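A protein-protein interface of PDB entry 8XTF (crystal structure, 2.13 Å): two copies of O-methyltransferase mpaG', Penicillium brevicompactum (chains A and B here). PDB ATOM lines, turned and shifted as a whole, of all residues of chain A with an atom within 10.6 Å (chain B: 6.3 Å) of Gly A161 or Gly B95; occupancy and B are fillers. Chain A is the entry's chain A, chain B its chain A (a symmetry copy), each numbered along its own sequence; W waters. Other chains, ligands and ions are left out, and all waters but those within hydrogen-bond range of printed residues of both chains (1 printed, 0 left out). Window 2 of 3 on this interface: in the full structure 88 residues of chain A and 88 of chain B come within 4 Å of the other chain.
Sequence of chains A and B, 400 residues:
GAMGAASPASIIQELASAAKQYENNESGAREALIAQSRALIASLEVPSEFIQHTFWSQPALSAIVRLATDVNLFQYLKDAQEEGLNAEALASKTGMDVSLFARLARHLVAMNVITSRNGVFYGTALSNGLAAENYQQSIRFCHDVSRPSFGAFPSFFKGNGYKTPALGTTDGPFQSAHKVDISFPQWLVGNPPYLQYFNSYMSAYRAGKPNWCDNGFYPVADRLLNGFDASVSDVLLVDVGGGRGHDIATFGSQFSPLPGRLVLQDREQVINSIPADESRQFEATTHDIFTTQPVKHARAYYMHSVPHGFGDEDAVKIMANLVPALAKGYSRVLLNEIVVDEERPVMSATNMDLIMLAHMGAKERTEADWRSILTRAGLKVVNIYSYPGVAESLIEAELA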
ATOM      1  N   PHE A 153      25.132  13.561  20.653  1.00  0.00           N
ATOM      2  CA  PHE A 153      24.371  14.782  20.370  1.00  0.00           C
ATOM      3  C   PHE A 153      24.671  15.385  18.997  1.00  0.00           C
ATOM      4  O   PHE A 153      23.718  15.668  18.255  1.00  0.00           O
ATOM      5  CB  PHE A 153      24.630  15.844  21.448  1.00  0.00           C
ATOM      6  CG  PHE A 153      23.690  15.801  22.616  1.00  0.00           C
ATOM      7  CD1 PHE A 153      23.222  14.592  23.111  1.00  0.00           C
ATOM      8  CD2 PHE A 153      23.337  16.967  23.271  1.00  0.00           C
ATOM      9  CE1 PHE A 153      22.399  14.553  24.201  1.00  0.00           C
ATOM     10  CE2 PHE A 153      22.516  16.937  24.374  1.00  0.00           C
ATOM     11  CZ  PHE A 153      22.043  15.725  24.840  1.00  0.00           C
ATOM     12  N   PRO A 154      25.929  15.632  18.608  1.00  0.00           N
ATOM     13  CA  PRO A 154      26.148  16.275  17.299  1.00  0.00           C
ATOM     14  C   PRO A 154      25.542  15.493  16.155  1.00  0.00           C
ATOM     15  O   PRO A 154      24.818  16.067  15.331  1.00  0.00           O
ATOM     16  CB  PRO A 154      27.677  16.360  17.193  1.00  0.00           C
ATOM     17  CG  PRO A 154      28.158  16.296  18.612  1.00  0.00           C
ATOM     18  CD  PRO A 154      27.199  15.387  19.316  1.00  0.00           C
ATOM     19  N   SER A 155      25.794  14.190  16.095  1.00  0.00           N
ATOM     20  CA  SER A 155      25.300  13.406  14.971  1.00  0.00           C
ATOM     21  C   SER A 155      23.803  13.121  15.080  1.00  0.00           C
ATOM     22  O   SER A 155      23.123  13.030  14.055  1.00  0.00           O
ATOM     23  CB  SER A 155      26.096  12.106  14.857  1.00  0.00           C
ATOM     24  OG  SER A 155      25.741  11.220  15.906  1.00  0.00           O
ATOM     25  N   PHE A 156      23.268  12.971  16.289  1.00  0.00           N
ATOM     26  CA  PHE A 156      21.844  12.690  16.398  1.00  0.00           C
ATOM     27  C   PHE A 156      21.015  13.882  15.929  1.00  0.00           C
ATOM     28  O   PHE A 156      20.078  13.728  15.139  1.00  0.00           O
ATOM     29  CB  PHE A 156      21.457  12.319  17.833  1.00  0.00           C
ATOM     30  CG  PHE A 156      19.981  12.219  18.020  1.00  0.00           C
ATOM     31  CD1 PHE A 156      19.289  11.093  17.580  1.00  0.00           C
ATOM     32  CD2 PHE A 156      19.269  13.273  18.551  1.00  0.00           C
ATOM     33  CE1 PHE A 156      17.906  11.008  17.710  1.00  0.00           C
ATOM     34  CE2 PHE A 156      17.904  13.205  18.679  1.00  0.00           C
ATOM     35  CZ  PHE A 156      17.215  12.064  18.262  1.00  0.00           C
ATOM     36  N   PHE A 157      21.346  15.080  16.408  1.00  0.00           N
ATOM     37  CA  PHE A 157      20.534  16.241  16.065  1.00  0.00           C
ATOM     38  C   PHE A 157      20.749  16.672  14.625  1.00  0.00           C
ATOM     39  O   PHE A 157      19.826  17.201  13.999  1.00  0.00           O
ATOM     40  CB  PHE A 157      20.802  17.370  17.059  1.00  0.00           C
ATOM     41  CG  PHE A 157      20.163  17.113  18.386  1.00  0.00           C
ATOM     42  CD1 PHE A 157      18.780  17.071  18.494  1.00  0.00           C
ATOM     43  CD2 PHE A 157      20.931  16.811  19.498  1.00  0.00           C
ATOM     44  CE1 PHE A 157      18.170  16.775  19.707  1.00  0.00           C
ATOM     45  CE2 PHE A 157      20.336  16.514  20.714  1.00  0.00           C
ATOM     46  CZ  PHE A 157      18.951  16.497  20.823  1.00  0.00           C
ATOM     47  N   LYS A 158      21.941  16.434  14.070  1.00  0.00           N
ATOM     48  CA  LYS A 158      22.103  16.642  12.635  1.00  0.00           C
ATOM     49  C   LYS A 158      21.178  15.712  11.853  1.00  0.00           C
ATOM     50  O   LYS A 158      20.494  16.145  10.916  1.00  0.00           O
ATOM     51  CB  LYS A 158      23.567  16.443  12.235  1.00  0.00           C
ATOM     52  CG  LYS A 158      23.793  16.430  10.733  1.00  0.00           C
ATOM     53  CD  LYS A 158      25.261  16.398  10.373  1.00  0.00           C
ATOM     54  CE  LYS A 158      25.456  16.932   8.956  1.00  0.00           C
ATOM     55  NZ  LYS A 158      26.707  16.438   8.299  1.00  0.00           N
ATOM     56  N   GLY A 159      21.104  14.447  12.262  1.00  0.00           N
ATOM     57  CA  GLY A 159      20.242  13.499  11.580  1.00  0.00           C
ATOM     58  C   GLY A 159      18.758  13.774  11.745  1.00  0.00           C
ATOM     59  O   GLY A 159      17.976  13.500  10.835  1.00  0.00           O
ATOM     60  N   ASN A 160      18.341  14.298  12.897  1.00  0.00           N
ATOM     61  CA  ASN A 160      16.913  14.505  13.119  1.00  0.00           C
ATOM     62  C   ASN A 160      16.467  15.913  12.735  1.00  0.00           C
ATOM     63  O   ASN A 160      15.345  16.308  13.065  1.00  0.00           O
ATOM     64  CB  ASN A 160      16.547  14.165  14.582  1.00  0.00           C
ATOM     65  CG  ASN A 160      16.503  15.386  15.511  1.00  0.00           C
ATOM     66  OD1 ASN A 160      17.251  16.338  15.358  1.00  0.00           O
ATOM     67  ND2 ASN A 160      15.644  15.320  16.510  1.00  0.00           N
ATOM     68  N   GLY A 161      17.321  16.678  12.052  1.00  0.00           N
ATOM     69  CA  GLY A 161      16.961  18.014  11.624  1.00  0.00           C
ATOM     70  C   GLY A 161      16.993  19.069  12.705  1.00  0.00           C
ATOM     71  O   GLY A 161      16.377  20.125  12.537  1.00  0.00           O
ATOM     72  N   TYR A 162      17.691  18.813  13.819  1.00  0.00           N
ATOM     73  CA  TYR A 162      17.794  19.754  14.941  1.00  0.00           C
ATOM     74  C   TYR A 162      16.419  20.052  15.540  1.00  0.00           C
ATOM     75  O   TYR A 162      16.040  21.207  15.761  1.00  0.00           O
ATOM     76  CB  TYR A 162      18.524  21.037  14.529  1.00  0.00           C
ATOM     77  CG  TYR A 162      19.936  20.754  14.046  1.00  0.00           C
ATOM     78  CD1 TYR A 162      20.965  20.512  14.955  1.00  0.00           C
ATOM     79  CD2 TYR A 162      20.232  20.690  12.687  1.00  0.00           C
ATOM     80  CE1 TYR A 162      22.256  20.241  14.526  1.00  0.00           C
ATOM     81  CE2 TYR A 162      21.527  20.408  12.241  1.00  0.00           C
ATOM     82  CZ  TYR A 162      22.535  20.189  13.167  1.00  0.00           C
ATOM     83  OH  TYR A 162      23.826  19.892  12.744  1.00  0.00           O
ATOM     84  N   LYS A 163      15.680  18.984  15.820  1.00  0.00           N
ATOM     85  CA  LYS A 163      14.353  19.056  16.409  1.00  0.00           C
ATOM     86  C   LYS A 163      14.379  18.517  17.835  1.00  0.00           C
ATOM     87  O   LYS A 163      15.127  17.586  18.158  1.00  0.00           O
ATOM     88  CB  LYS A 163      13.342  18.263  15.575  1.00  0.00           C
ATOM     89  CG  LYS A 163      13.280  18.687  14.129  1.00  0.00           C
ATOM     90  CD  LYS A 163      12.583  20.020  13.983  1.00  0.00           C
ATOM     91  CE  LYS A 163      12.017  20.206  12.581  1.00  0.00           C
ATOM     92  NZ  LYS A 163      11.764  18.887  11.930  1.00  0.00           N
ATOM     93  N   THR A 164      13.575  19.132  18.693  1.00  0.00           N
ATOM     94  CA  THR A 164      13.314  18.552  20.008  1.00  0.00           C
ATOM     95  C   THR A 164      12.676  17.172  19.815  1.00  0.00           C
ATOM     96  O   THR A 164      11.778  17.029  18.979  1.00  0.00           O
ATOM     97  CB  THR A 164      12.400  19.483  20.822  1.00  0.00           C
ATOM     98  OG1 THR A 164      13.132  20.660  21.195  1.00  0.00           O
ATOM     99  CG2 THR A 164      11.892  18.796  22.102  1.00  0.00           C
ATOM    100  N   PRO A 165      13.156  16.118  20.515  1.00  0.00           N
ATOM    101  CA  PRO A 165      12.513  14.796  20.411  1.00  0.00           C
ATOM    102  C   PRO A 165      10.998  14.853  20.566  1.00  0.00           C
ATOM    103  O   PRO A 165      10.501  15.250  21.624  1.00  0.00           O
ATOM    104  CB  PRO A 165      13.162  14.016  21.559  1.00  0.00           C
ATOM    105  CG  PRO A 165      14.526  14.612  21.659  1.00  0.00           C
ATOM    106  CD  PRO A 165      14.341  16.086  21.394  1.00  0.00           C
ATOM    107  N   ALA A 166      10.253  14.473  19.527  1.00  0.00           N
ATOM    108  CA  ALA A 166       8.798  14.638  19.554  1.00  0.00           C
ATOM    109  C   ALA A 166       8.144  13.716  20.578  1.00  0.00           C
ATOM    110  O   ALA A 166       7.304  14.153  21.372  1.00  0.00           O
ATOM    111  CB  ALA A 166       8.208  14.395  18.165  1.00  0.00           C
ATOM    112  N   ASP A 171      12.707   8.424  20.783  1.00  0.00           N
ATOM    113  CA  ASP A 171      13.253   9.126  19.623  1.00  0.00           C
ATOM    114  C   ASP A 171      14.295  10.168  20.030  1.00  0.00           C
ATOM    115  O   ASP A 171      14.332  11.275  19.490  1.00  0.00           O
ATOM    116  CB  ASP A 171      12.134   9.783  18.806  1.00  0.00           C
ATOM    117  CG  ASP A 171      11.284  10.759  19.633  1.00  0.00           C
ATOM    118  OD1 ASP A 171      11.453  10.809  20.869  1.00  0.00           O
ATOM    119  OD2 ASP A 171      10.433  11.467  19.043  1.00  0.00           O
ATOM    120  N   VAL B  71      26.630  24.138  12.720  1.00  0.00           N
ATOM    121  CA  VAL B  71      25.569  25.091  12.426  1.00  0.00           C
ATOM    122  C   VAL B  71      26.077  26.524  12.388  1.00  0.00           C
ATOM    123  O   VAL B  71      25.268  27.460  12.386  1.00  0.00           O
ATOM    124  CB  VAL B  71      24.403  24.974  13.430  1.00  0.00           C
ATOM    125  CG1 VAL B  71      23.754  23.596  13.347  1.00  0.00           C
ATOM    126  CG2 VAL B  71      24.890  25.289  14.846  1.00  0.00           C
ATOM    127  N   LEU B  90      18.763  33.365  16.145  1.00  0.00           N
ATOM    128  CA  LEU B  90      19.839  32.395  16.000  1.00  0.00           C
ATOM    129  C   LEU B  90      19.312  31.040  15.565  1.00  0.00           C
ATOM    130  O   LEU B  90      19.956  30.344  14.770  1.00  0.00           O
ATOM    131  CB  LEU B  90      20.596  32.260  17.312  1.00  0.00           C
ATOM    132  CG  LEU B  90      21.793  33.189  17.378  1.00  0.00           C
ATOM    133  CD1 LEU B  90      22.228  33.337  18.828  1.00  0.00           C
ATOM    134  CD2 LEU B  90      22.910  32.649  16.484  1.00  0.00           C
ATOM    135  N   ALA B  91      18.153  30.634  16.089  1.00  0.00           N
ATOM    136  CA  ALA B  91      17.560  29.375  15.657  1.00  0.00           C
ATOM    137  C   ALA B  91      17.229  29.417  14.176  1.00  0.00           C
ATOM    138  O   ALA B  91      17.419  28.430  13.457  1.00  0.00           O
ATOM    139  CB  ALA B  91      16.307  29.069  16.473  1.00  0.00           C
ATOM    140  N   SER B  92      16.733  30.556  13.705  1.00  0.00           N
ATOM    141  CA  SER B  92      16.413  30.719  12.294  1.00  0.00           C
ATOM    142  C   SER B  92      17.668  30.641  11.435  1.00  0.00           C
ATOM    143  O   SER B  92      17.669  29.980  10.391  1.00  0.00           O
ATOM    144  CB  SER B  92      15.680  32.046  12.099  1.00  0.00           C
ATOM    145  OG  SER B  92      15.537  32.366  10.736  1.00  0.00           O
ATOM    146  N   LYS B  93      18.753  31.290  11.873  1.00  0.00           N
ATOM    147  CA  LYS B  93      20.013  31.251  11.131  1.00  0.00           C
ATOM    148  C   LYS B  93      20.629  29.858  11.137  1.00  0.00           C
ATOM    149  O   LYS B  93      21.152  29.405  10.120  1.00  0.00           O
ATOM    150  CB  LYS B  93      21.009  32.250  11.714  1.00  0.00           C
ATOM    151  CG  LYS B  93      20.700  33.696  11.379  1.00  0.00           C
ATOM    152  CD  LYS B  93      21.442  34.638  12.315  1.00  0.00           C
ATOM    153  CE  LYS B  93      22.168  35.700  11.549  1.00  0.00           C
ATOM    154  NZ  LYS B  93      21.273  36.356  10.563  1.00  0.00           N
ATOM    155  N   THR B  94      20.594  29.168  12.275  1.00  0.00           N
ATOM    156  CA  THR B  94      21.235  27.862  12.342  1.00  0.00           C
ATOM    157  C   THR B  94      20.348  26.733  11.839  1.00  0.00           C
ATOM    158  O   THR B  94      20.829  25.601  11.722  1.00  0.00           O
ATOM    159  CB  THR B  94      21.677  27.565  13.777  1.00  0.00           C
ATOM    160  OG1 THR B  94      20.531  27.564  14.636  1.00  0.00           O
ATOM    161  CG2 THR B  94      22.672  28.608  14.257  1.00  0.00           C
ATOM    162  N   GLY B  95      19.085  27.009  11.532  1.00  0.00           N
ATOM    163  CA  GLY B  95      18.162  25.960  11.131  1.00  0.00           C
ATOM    164  C   GLY B  95      17.777  25.006  12.246  1.00  0.00           C
ATOM    165  O   GLY B  95      17.539  23.820  11.985  1.00  0.00           O
ATOM    166  N   MET B  96      17.701  25.495  13.480  1.00  0.00           N
ATOM    167  CA  MET B  96      17.425  24.675  14.647  1.00  0.00           C
ATOM    168  C   MET B  96      16.060  25.013  15.231  1.00  0.00           C
ATOM    169  O   MET B  96      15.611  26.152  15.171  1.00  0.00           O
ATOM    170  CB  MET B  96      18.480  24.909  15.725  1.00  0.00           C
ATOM    171  CG  MET B  96      19.868  24.478  15.328  1.00  0.00           C
ATOM    172  SD  MET B  96      21.012  24.664  16.708  1.00  0.00           S
ATOM    173  CE  MET B  96      20.450  23.322  17.764  1.00  0.00           C
ATOM    174  N   ASP B  97      15.422  24.010  15.826  1.00  0.00           N
ATOM    175  CA  ASP B  97      14.280  24.252  16.695  1.00  0.00           C
ATOM    176  C   ASP B  97      14.635  25.320  17.729  1.00  0.00           C
ATOM    177  O   ASP B  97      15.690  25.251  18.366  1.00  0.00           O
ATOM    178  CB  ASP B  97      13.895  22.939  17.381  1.00  0.00           C
ATOM    179  CG  ASP B  97      12.428  22.856  17.734  1.00  0.00           C
ATOM    180  OD1 ASP B  97      11.925  23.788  18.399  1.00  0.00           O
ATOM    181  OD2 ASP B  97      11.786  21.842  17.357  1.00  0.00           O
HETATM  182  O   HOH W   1      14.510  22.704  12.947  1.00  0.00           O
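The backbone NH (N) of Asp B97 is in hydrogen-bond range of the backbone carbonyl oxygen (O) of Tyr A162 (2.9 Å).
O of Phe A157 sits at hydrogen-bond distance from N of Tyr A162 (2.7 Å).
OD1 of Asn A160 is in hydrogen-bond range of N of Tyr A162 (2.9 Å).
The side-chain amide nitrogen (ND2) of Asn A160 sits at hydrogen-bond distance from the backbone carbonyl oxygen (O) of Lys A163 (2.8 Å).
The backbone carbonyl oxygen (O) of Ala B91 lies within hydrogen-bond range of the backbone NH (N) of Met B96 (2.9 Å).
OG1 of Thr B94 sits close to SD of Met B96, at 3.6 Å.
Gly B95 touches Gly A161 (O to O, 3.9 Å).
Val B71 touches Tyr A162 (CG1 to CZ, 3.6 Å).
Tyr A162 touches Gly B95 (CB to O, 3.9 Å).
Tyr A162 touches Met B96 (CB to CG, 3.8 Å).
Lys A163 touches Asp B97 (CA to OD2, 3.9 Å).
OD2 of Asp B97 touches N of Thr A164, 3.5 Å away.
Phe A157 touches none of the printed residues of chain B.
Gly A161 touches one residue of chain B.
Of the printed residues of chain B, Tyr A162 touches Val B71 (3.6 Å), Gly B95 (3.9 Å), Met B96 (3.8 Å) and Asp B97 (2.9 Å).
Printed residues of chain B within 4 Å of Lys A163: Asp B97 (3.9 Å).
Asp A171 touches none of the printed residues of chain B.
Printed residues of chain A within 4 Å of Val B71: Tyr A162 (3.6 Å).
No residue of chain A comes within 4 Å of Ala B91.
No residue of chain A comes within 4 Å of Thr B94.
Gly B95 touches just these residues of chain A: Gly A161 and Tyr A162.
Of chain A, only Tyr A162 (3.8 Å) comes within 4 Å of Met B96.
Of the printed residues of chain A, Asp B97 touches Tyr A162, Lys A163 and Thr A164.
The nearest printed residue of chain B that does not touch Thr A164 is Met B96 (7.3 Å).
Among the printed residues, no Asp or Glu carboxylate lies within 4 Å of a Lys or Arg side-chain nitrogen of the other chain.
No position is printed for both chains.
Of the 7 pairs that touch across the chains among the printed residues, none has its exchanged pair printed and touching as well.
Water W1 lies within hydrogen-bond range of O of Gly A161 (3.2 Å), N of Asp B97 (3.3 Å) and O of Gly B95 (3.4 Å).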
